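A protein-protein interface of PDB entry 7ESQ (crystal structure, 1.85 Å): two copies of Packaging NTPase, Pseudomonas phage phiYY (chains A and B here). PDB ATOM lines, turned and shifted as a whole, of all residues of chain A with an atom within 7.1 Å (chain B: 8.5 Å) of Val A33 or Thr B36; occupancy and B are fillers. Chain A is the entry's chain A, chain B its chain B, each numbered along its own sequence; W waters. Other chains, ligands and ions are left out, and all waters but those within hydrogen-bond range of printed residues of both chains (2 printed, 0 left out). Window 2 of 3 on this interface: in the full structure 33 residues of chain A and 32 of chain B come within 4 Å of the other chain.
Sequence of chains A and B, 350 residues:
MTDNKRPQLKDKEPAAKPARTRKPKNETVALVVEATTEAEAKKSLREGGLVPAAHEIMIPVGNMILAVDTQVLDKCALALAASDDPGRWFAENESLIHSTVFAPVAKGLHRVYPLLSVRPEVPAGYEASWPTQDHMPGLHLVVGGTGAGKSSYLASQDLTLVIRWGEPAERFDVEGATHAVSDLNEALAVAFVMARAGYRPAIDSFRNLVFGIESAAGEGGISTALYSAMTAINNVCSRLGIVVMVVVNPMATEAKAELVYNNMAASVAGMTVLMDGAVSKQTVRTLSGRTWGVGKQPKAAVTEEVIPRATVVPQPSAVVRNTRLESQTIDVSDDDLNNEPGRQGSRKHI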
ATOM      1  N   ALA A  30       9.102  21.394  22.730  1.00  0.00           N
ATOM      2  CA  ALA A  30      10.304  20.579  22.566  1.00  0.00           C
ATOM      3  C   ALA A  30      10.055  19.172  23.102  1.00  0.00           C
ATOM      4  O   ALA A  30       9.598  18.995  24.241  1.00  0.00           O
ATOM      5  CB  ALA A  30      11.498  21.220  23.282  1.00  0.00           C
ATOM      6  N   LEU A  31      10.376  18.172  22.280  1.00  0.00           N
ATOM      7  CA  LEU A  31      10.111  16.775  22.611  1.00  0.00           C
ATOM      8  C   LEU A  31      11.349  15.996  23.019  1.00  0.00           C
ATOM      9  O   LEU A  31      11.224  15.006  23.755  1.00  0.00           O
ATOM     10  CB  LEU A  31       9.463  16.057  21.421  1.00  0.00           C
ATOM     11  CG  LEU A  31       8.146  16.619  20.907  1.00  0.00           C
ATOM     12  CD1 LEU A  31       7.749  15.919  19.608  1.00  0.00           C
ATOM     13  CD2 LEU A  31       7.077  16.467  21.977  1.00  0.00           C
ATOM     14  N   VAL A  32      12.541  16.398  22.574  1.00  0.00           N
ATOM     15  CA  VAL A  32      13.711  15.584  22.881  1.00  0.00           C
ATOM     16  C   VAL A  32      14.941  16.406  23.269  1.00  0.00           C
ATOM     17  O   VAL A  32      15.815  15.901  23.976  1.00  0.00           O
ATOM     18  CB  VAL A  32      14.033  14.641  21.704  1.00  0.00           C
ATOM     19  CG1 VAL A  32      14.539  15.419  20.518  1.00  0.00           C
ATOM     20  CG2 VAL A  32      15.063  13.602  22.130  1.00  0.00           C
ATOM     21  N   VAL A  33      15.038  17.666  22.833  1.00  0.00           N
ATOM     22  CA  VAL A  33      16.215  18.482  23.140  1.00  0.00           C
ATOM     23  C   VAL A  33      15.924  19.331  24.372  1.00  0.00           C
ATOM     24  O   VAL A  33      15.035  20.192  24.351  1.00  0.00           O
ATOM     25  CB  VAL A  33      16.629  19.367  21.954  1.00  0.00           C
ATOM     26  CG1 VAL A  33      17.882  20.180  22.331  1.00  0.00           C
ATOM     27  CG2 VAL A  33      16.897  18.513  20.730  1.00  0.00           C
ATOM     28  N   GLU A  34      16.672  19.088  25.440  1.00  0.00           N
ATOM     29  CA  GLU A  34      16.543  19.826  26.690  1.00  0.00           C
ATOM     30  C   GLU A  34      17.781  20.677  26.941  1.00  0.00           C
ATOM     31  O   GLU A  34      18.822  20.511  26.305  1.00  0.00           O
ATOM     32  CB  GLU A  34      16.335  18.890  27.882  1.00  0.00           C
ATOM     33  CG  GLU A  34      17.514  17.980  28.131  1.00  0.00           C
ATOM     34  CD  GLU A  34      17.262  16.996  29.256  1.00  0.00           C
ATOM     35  OE1 GLU A  34      16.879  17.450  30.364  1.00  0.00           O
ATOM     36  OE2 GLU A  34      17.392  15.771  29.023  1.00  0.00           O
ATOM     37  N   ALA A  35      17.653  21.580  27.913  1.00  0.00           N
ATOM     38  CA  ALA A  35      18.726  22.512  28.235  1.00  0.00           C
ATOM     39  C   ALA A  35      19.946  21.769  28.753  1.00  0.00           C
ATOM     40  O   ALA A  35      19.834  20.852  29.569  1.00  0.00           O
ATOM     41  CB  ALA A  35      18.255  23.521  29.283  1.00  0.00           C
ATOM     42  N   THR A  36      21.122  22.170  28.272  1.00  0.00           N
ATOM     43  CA  THR A  36      22.380  21.656  28.788  1.00  0.00           C
ATOM     44  C   THR A  36      23.326  22.758  29.251  1.00  0.00           C
ATOM     45  O   THR A  36      24.422  22.453  29.729  1.00  0.00           O
ATOM     46  CB  THR A  36      23.076  20.792  27.728  1.00  0.00           C
ATOM     47  OG1 THR A  36      23.399  21.607  26.596  1.00  0.00           O
ATOM     48  CG2 THR A  36      22.188  19.640  27.288  1.00  0.00           C
ATOM     49  N   GLU A  40      20.369  28.096  28.415  1.00  0.00           N
ATOM     50  CA  GLU A  40      19.212  27.337  27.955  1.00  0.00           C
ATOM     51  C   GLU A  40      18.257  27.006  29.103  1.00  0.00           C
ATOM     52  O   GLU A  40      17.033  26.975  28.900  1.00  0.00           O
ATOM     53  CB  GLU A  40      19.680  26.064  27.258  1.00  0.00           C
ATOM     54  CG  GLU A  40      20.385  26.330  25.937  1.00  0.00           C
ATOM     55  CD  GLU A  40      21.113  25.117  25.394  1.00  0.00           C
ATOM     56  OE1 GLU A  40      21.723  25.237  24.310  1.00  0.00           O
ATOM     57  OE2 GLU A  40      21.079  24.041  26.033  1.00  0.00           O
ATOM     58  N   ARG A  46       8.185  24.929  27.662  1.00  0.00           N
ATOM     59  CA  ARG A  46       7.883  24.596  26.272  1.00  0.00           C
ATOM     60  C   ARG A  46       9.157  24.450  25.455  1.00  0.00           C
ATOM     61  O   ARG A  46       9.276  23.555  24.612  1.00  0.00           O
ATOM     62  CB  ARG A  46       6.993  25.690  25.663  1.00  0.00           C
ATOM     63  CG  ARG A  46       6.751  25.540  24.158  1.00  0.00           C
ATOM     64  CD  ARG A  46       5.865  26.676  23.617  1.00  0.00           C
ATOM     65  NE  ARG A  46       4.583  26.719  24.321  1.00  0.00           N
ATOM     66  CZ  ARG A  46       3.505  26.018  23.972  1.00  0.00           C
ATOM     67  NH1 ARG A  46       3.523  25.244  22.894  1.00  0.00           N
ATOM     68  NH2 ARG A  46       2.401  26.099  24.694  1.00  0.00           N
ATOM     69  N   GLU A  47      10.131  25.308  25.713  1.00  0.00           N
ATOM     70  CA  GLU A  47      11.343  25.360  24.912  1.00  0.00           C
ATOM     71  C   GLU A  47      12.431  24.424  25.417  1.00  0.00           C
ATOM     72  O   GLU A  47      13.548  24.445  24.883  1.00  0.00           O
ATOM     73  CB  GLU A  47      11.873  26.789  24.908  1.00  0.00           C
ATOM     74  CG  GLU A  47      11.094  27.711  24.010  1.00  0.00           C
ATOM     75  CD  GLU A  47      11.552  29.148  24.185  1.00  0.00           C
ATOM     76  OE1 GLU A  47      11.012  29.850  25.073  1.00  0.00           O
ATOM     77  OE2 GLU A  47      12.458  29.572  23.438  1.00  0.00           O
ATOM     78  N   GLY A  48      12.158  23.628  26.447  1.00  0.00           N
ATOM     79  CA  GLY A  48      13.164  22.723  26.956  1.00  0.00           C
ATOM     80  C   GLY A  48      13.981  23.248  28.116  1.00  0.00           C
ATOM     81  O   GLY A  48      14.941  22.578  28.522  1.00  0.00           O
ATOM     82  N   GLY A  49      13.624  24.409  28.669  1.00  0.00           N
ATOM     83  CA  GLY A  49      14.271  24.943  29.849  1.00  0.00           C
ATOM     84  C   GLY A  49      13.624  24.457  31.139  1.00  0.00           C
ATOM     85  O   GLY A  49      12.745  23.591  31.152  1.00  0.00           O
ATOM     86  N   VAL A 105      10.198  18.536  28.571  1.00  0.00           N
ATOM     87  CA  VAL A 105      11.276  17.584  28.280  1.00  0.00           C
ATOM     88  C   VAL A 105      12.414  17.649  29.309  1.00  0.00           C
ATOM     89  O   VAL A 105      13.100  16.647  29.525  1.00  0.00           O
ATOM     90  CB  VAL A 105      11.809  17.798  26.843  1.00  0.00           C
ATOM     91  CG1 VAL A 105      12.460  19.179  26.696  1.00  0.00           C
ATOM     92  CG2 VAL A 105      12.820  16.681  26.439  1.00  0.00           C
ATOM     93  N   ALA A 106      12.639  18.791  29.969  1.00  0.00           N
ATOM     94  CA  ALA A 106      13.793  18.922  30.855  1.00  0.00           C
ATOM     95  C   ALA A 106      13.696  17.987  32.060  1.00  0.00           C
ATOM     96  O   ALA A 106      12.677  17.949  32.757  1.00  0.00           O
ATOM     97  CB  ALA A 106      13.951  20.370  31.328  1.00  0.00           C
ATOM     98  N   LYS A 107      14.785  17.269  32.332  1.00  0.00           N
ATOM     99  CA  LYS A 107      14.767  16.238  33.366  1.00  0.00           C
ATOM    100  C   LYS A 107      14.927  16.793  34.779  1.00  0.00           C
ATOM    101  O   LYS A 107      14.431  16.178  35.731  1.00  0.00           O
ATOM    102  CB  LYS A 107      15.857  15.198  33.092  1.00  0.00           C
ATOM    103  CG  LYS A 107      15.763  14.493  31.744  1.00  0.00           C
ATOM    104  CD  LYS A 107      14.317  14.120  31.407  1.00  0.00           C
ATOM    105  CE  LYS A 107      14.212  13.384  30.067  1.00  0.00           C
ATOM    106  NZ  LYS A 107      14.318  14.306  28.901  1.00  0.00           N
ATOM    107  N   VAL B  32      17.097   0.623  16.616  1.00  0.00           N
ATOM    108  CA  VAL B  32      18.160   0.988  17.559  1.00  0.00           C
ATOM    109  C   VAL B  32      18.239   2.497  17.614  1.00  0.00           C
ATOM    110  O   VAL B  32      18.509   3.074  18.667  1.00  0.00           O
ATOM    111  CB  VAL B  32      19.564   0.513  17.124  1.00  0.00           C
ATOM    112  CG1 VAL B  32      20.685   1.003  18.130  1.00  0.00           C
ATOM    113  CG2 VAL B  32      19.608  -0.927  16.677  1.00  0.00           C
ATOM    114  N   VAL B  33      18.082   3.127  16.451  1.00  0.00           N
ATOM    115  CA  VAL B  33      18.343   4.557  16.276  1.00  0.00           C
ATOM    116  C   VAL B  33      17.049   5.347  16.467  1.00  0.00           C
ATOM    117  O   VAL B  33      16.098   5.201  15.690  1.00  0.00           O
ATOM    118  CB  VAL B  33      18.953   4.859  14.898  1.00  0.00           C
ATOM    119  CG1 VAL B  33      19.370   6.315  14.830  1.00  0.00           C
ATOM    120  CG2 VAL B  33      20.162   3.970  14.644  1.00  0.00           C
ATOM    121  N   GLU B  34      17.021   6.202  17.479  1.00  0.00           N
ATOM    122  CA  GLU B  34      15.851   7.015  17.783  1.00  0.00           C
ATOM    123  C   GLU B  34      16.160   8.493  17.586  1.00  0.00           C
ATOM    124  O   GLU B  34      17.315   8.897  17.433  1.00  0.00           O
ATOM    125  CB  GLU B  34      15.379   6.786  19.212  1.00  0.00           C
ATOM    126  CG  GLU B  34      16.433   7.162  20.220  1.00  0.00           C
ATOM    127  CD  GLU B  34      16.042   6.775  21.626  1.00  0.00           C
ATOM    128  OE1 GLU B  34      14.951   7.210  22.068  1.00  0.00           O
ATOM    129  OE2 GLU B  34      16.783   5.982  22.247  1.00  0.00           O
ATOM    130  N   ALA B  35      15.101   9.300  17.613  1.00  0.00           N
ATOM    131  CA  ALA B  35      15.242  10.732  17.381  1.00  0.00           C
ATOM    132  C   ALA B  35      16.158  11.353  18.426  1.00  0.00           C
ATOM    133  O   ALA B  35      16.037  11.069  19.618  1.00  0.00           O
ATOM    134  CB  ALA B  35      13.872  11.405  17.417  1.00  0.00           C
ATOM    135  N   THR B  36      17.086  12.196  17.975  1.00  0.00           N
ATOM    136  CA  THR B  36      17.879  13.007  18.887  1.00  0.00           C
ATOM    137  C   THR B  36      17.748  14.507  18.637  1.00  0.00           C
ATOM    138  O   THR B  36      18.268  15.292  19.436  1.00  0.00           O
ATOM    139  CB  THR B  36      19.361  12.605  18.820  1.00  0.00           C
ATOM    140  OG1 THR B  36      19.868  12.900  17.515  1.00  0.00           O
ATOM    141  CG2 THR B  36      19.532  11.112  19.105  1.00  0.00           C
ATOM    142  N   THR B  37      17.056  14.922  17.575  1.00  0.00           N
ATOM    143  CA  THR B  37      16.764  16.317  17.285  1.00  0.00           C
ATOM    144  C   THR B  37      15.259  16.516  17.185  1.00  0.00           C
ATOM    145  O   THR B  37      14.494  15.561  17.012  1.00  0.00           O
ATOM    146  CB  THR B  37      17.412  16.768  15.971  1.00  0.00           C
ATOM    147  OG1 THR B  37      16.689  16.208  14.870  1.00  0.00           O
ATOM    148  CG2 THR B  37      18.850  16.315  15.905  1.00  0.00           C
ATOM    149  N   GLU B  38      14.827  17.777  17.287  1.00  0.00           N
ATOM    150  CA  GLU B  38      13.395  18.040  17.218  1.00  0.00           C
ATOM    151  C   GLU B  38      12.823  17.684  15.857  1.00  0.00           C
ATOM    152  O   GLU B  38      11.688  17.205  15.776  1.00  0.00           O
ATOM    153  CB  GLU B  38      13.088  19.498  17.565  1.00  0.00           C
ATOM    154  CG  GLU B  38      13.495  19.840  18.988  1.00  0.00           C
ATOM    155  CD  GLU B  38      12.674  19.045  20.012  1.00  0.00           C
ATOM    156  OE1 GLU B  38      13.246  18.620  21.037  1.00  0.00           O
ATOM    157  OE2 GLU B  38      11.459  18.831  19.777  1.00  0.00           O
ATOM    158  N   ALA B  39      13.591  17.891  14.782  1.00  0.00           N
ATOM    159  CA  ALA B  39      13.102  17.516  13.460  1.00  0.00           C
ATOM    160  C   ALA B  39      12.877  16.013  13.365  1.00  0.00           C
ATOM    161  O   ALA B  39      11.860  15.562  12.820  1.00  0.00           O
ATOM    162  CB  ALA B  39      14.081  17.974  12.380  1.00  0.00           C
ATOM    163  N   GLU B  40      13.814  15.221  13.890  1.00  0.00           N
ATOM    164  CA  GLU B  40      13.648  13.768  13.911  1.00  0.00           C
ATOM    165  C   GLU B  40      12.520  13.330  14.843  1.00  0.00           C
ATOM    166  O   GLU B  40      11.847  12.328  14.572  1.00  0.00           O
ATOM    167  CB  GLU B  40      14.947  13.101  14.345  1.00  0.00           C
ATOM    168  CG  GLU B  40      16.035  13.065  13.275  1.00  0.00           C
ATOM    169  CD  GLU B  40      17.398  12.675  13.840  1.00  0.00           C
ATOM    170  OE1 GLU B  40      18.383  12.694  13.072  1.00  0.00           O
ATOM    171  OE2 GLU B  40      17.500  12.371  15.053  1.00  0.00           O
ATOM    172  N   ALA B  41      12.322  14.034  15.957  1.00  0.00           N
ATOM    173  CA  ALA B  41      11.276  13.651  16.901  1.00  0.00           C
ATOM    174  C   ALA B  41       9.884  13.751  16.293  1.00  0.00           C
ATOM    175  O   ALA B  41       8.956  13.080  16.771  1.00  0.00           O
ATOM    176  CB  ALA B  41      11.369  14.508  18.169  1.00  0.00           C
ATOM    177  N   LYS B  42       9.712  14.569  15.250  1.00  0.00           N
ATOM    178  CA  LYS B  42       8.402  14.741  14.635  1.00  0.00           C
ATOM    179  C   LYS B  42       8.040  13.618  13.677  1.00  0.00           C
ATOM    180  O   LYS B  42       6.899  13.587  13.192  1.00  0.00           O
ATOM    181  CB  LYS B  42       8.338  16.083  13.882  1.00  0.00           C
ATOM    182  CG  LYS B  42       8.290  17.302  14.804  1.00  0.00           C
ATOM    183  CD  LYS B  42       8.377  18.611  14.016  1.00  0.00           C
ATOM    184  CE  LYS B  42       8.135  19.811  14.932  1.00  0.00           C
ATOM    185  NZ  LYS B  42       7.061  20.733  14.427  1.00  0.00           N
ATOM    186  N   GLY B  48      11.327   5.941  14.313  1.00  0.00           N
ATOM    187  CA  GLY B  48      12.111   6.310  15.464  1.00  0.00           C
ATOM    188  C   GLY B  48      11.781   7.662  16.047  1.00  0.00           C
ATOM    189  O   GLY B  48      12.530   8.143  16.911  1.00  0.00           O
ATOM    190  N   GLY B  49      10.685   8.279  15.613  1.00  0.00           N
ATOM    191  CA  GLY B  49      10.226   9.535  16.163  1.00  0.00           C
ATOM    192  C   GLY B  49       9.245   9.332  17.298  1.00  0.00           C
ATOM    193  O   GLY B  49       9.012   8.218  17.774  1.00  0.00           O
ATOM    194  N   LEU B  50       8.666  10.446  17.746  1.00  0.00           N
ATOM    195  CA  LEU B  50       7.816  10.442  18.931  1.00  0.00           C
ATOM    196  C   LEU B  50       6.372  10.793  18.626  1.00  0.00           C
ATOM    197  O   LEU B  50       5.577  10.932  19.562  1.00  0.00           O
ATOM    198  CB  LEU B  50       8.362  11.407  19.994  1.00  0.00           C
ATOM    199  CG  LEU B  50       9.688  11.059  20.661  1.00  0.00           C
ATOM    200  CD1 LEU B  50      10.259  12.281  21.340  1.00  0.00           C
ATOM    201  CD2 LEU B  50       9.450  10.009  21.699  1.00  0.00           C
ATOM    202  N   ALA B 106      11.626   4.844  20.253  1.00  0.00           N
ATOM    203  CA  ALA B 106      11.900   6.113  20.934  1.00  0.00           C
ATOM    204  C   ALA B 106      11.577   6.029  22.425  1.00  0.00           C
ATOM    205  O   ALA B 106      10.494   5.584  22.803  1.00  0.00           O
ATOM    206  CB  ALA B 106      11.094   7.239  20.298  1.00  0.00           C
ATOM    207  N   ARG B 111       6.748   9.749  28.785  1.00  0.00           N
ATOM    208  CA  ARG B 111       6.683  11.135  29.231  1.00  0.00           C
ATOM    209  C   ARG B 111       5.752  11.955  28.351  1.00  0.00           C
ATOM    210  O   ARG B 111       4.927  12.732  28.851  1.00  0.00           O
ATOM    211  CB  ARG B 111       8.086  11.744  29.227  1.00  0.00           C
ATOM    212  CG  ARG B 111       8.143  13.085  29.938  1.00  0.00           C
ATOM    213  CD  ARG B 111       9.363  13.875  29.522  1.00  0.00           C
ATOM    214  NE  ARG B 111       9.130  14.562  28.250  1.00  0.00           N
ATOM    215  CZ  ARG B 111       9.775  14.278  27.123  1.00  0.00           C
ATOM    216  NH1 ARG B 111      10.687  13.312  27.108  1.00  0.00           N
ATOM    217  NH2 ARG B 111       9.514  14.963  26.013  1.00  0.00           N
HETATM  218  O   HOH W   1      12.215  12.646  24.765  1.00  0.00           O
HETATM  219  O   HOH W   2       7.936  17.220  25.710  1.00  0.00           O
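Val A32 touches Ala B35, but with the chains exchanged Ala A35 does not touch Val B32 (20.7 Å).
Val A32 touches Thr B36, but with the chains exchanged Thr A36 does not touch Val B32 (19.0 Å).
Val A33 touches Thr B36, but with the chains exchanged Thr A36 does not touch Val B33 (18.5 Å).
The backbone carbonyl oxygen (O) of Arg A46 is in hydrogen-bond range of the backbone NH (N) of Ala A30 (2.9 Å).
O of Ala B41 lies within hydrogen-bond range of N of Leu B50 (2.8 Å).
The backbone carbonyl oxygen of Gly B48 lies within hydrogen-bond range of the backbone NH of Ala B35 (2.9 Å).
The backbone NH (N) of Thr B36 sits at hydrogen-bond distance from the side-chain carboxylate (OE2) of Glu B40 (3.0 Å).
OG1 of Thr B37 is in hydrogen-bond range of N of Glu B40 (3.2 Å).
O of Val A105 sits at hydrogen-bond distance from NZ of Lys A107 (2.7 Å).
O of Leu A31 sits at hydrogen-bond distance from NH2 of Arg B111.
The backbone NH of Leu A31 lies within hydrogen-bond range of the side-chain carboxylate of Glu B38 (2.8 Å).
The backbone NH (N) of Val A33 sits at hydrogen-bond distance from the side-chain carboxylate (OE1) of Glu B38 (2.7 Å).
The side-chain carboxylate (OE1) of Glu B38 sits at hydrogen-bond distance from the backbone NH (N) of Val A32, at 2.8 Å.
Of the 16 printed residues of chain B, 6 touch a printed residue of chain A.
Hydrophobic or aromatic side chains of chain B that line the printed part of chain A: Leu B50.
Glu B38 touches Ala A30.
Leu A31 touches Leu B50 (O to CD1, 3.8 Å).
Val A32 touches Ala B35 (CG2 to O, 3.7 Å).
Thr B36 touches Val A32 (C to CG1, 3.8 Å).
Val A32 touches Thr B37 (CG1 to O, 3.5 Å).
Thr B36 touches Val A33 (O to CG2, 3.7 Å).
Arg B111 touches Val A105.
Water W1 lies within hydrogen-bond range of O of Leu A31 (2.8 Å) and NH1 of Arg B111 (2.9 Å).
Water W2 bridges NH2 of Arg B111 (2.8 Å) and O of Ala A30 (2.8 Å).
Val A33 touches just these residues of chain B: Thr B36 (3.7 Å) and Glu B38 (2.7 Å).
Of the printed residues of chain A, Thr B36 touches Val A32 (3.8 Å) and Val A33 (3.7 Å).
Val A32 touches just these residues of chain B: Ala B35, Thr B36, Thr B37 and Glu B38.
Of the printed residues of chain B, Leu A31 touches Glu B38 (2.8 Å), Leu B50 (3.8 Å) and Arg B111 (2.8 Å).
Of the printed residues of chain A, Ala B35 touches Val A32 (3.7 Å).
Lys B42 touches none of the printed residues of chain A.
Thr A36 touches none of the printed residues of chain B.
The nearest printed residue of chain A that does not touch Glu B38 is Glu A34 (5.6 Å).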
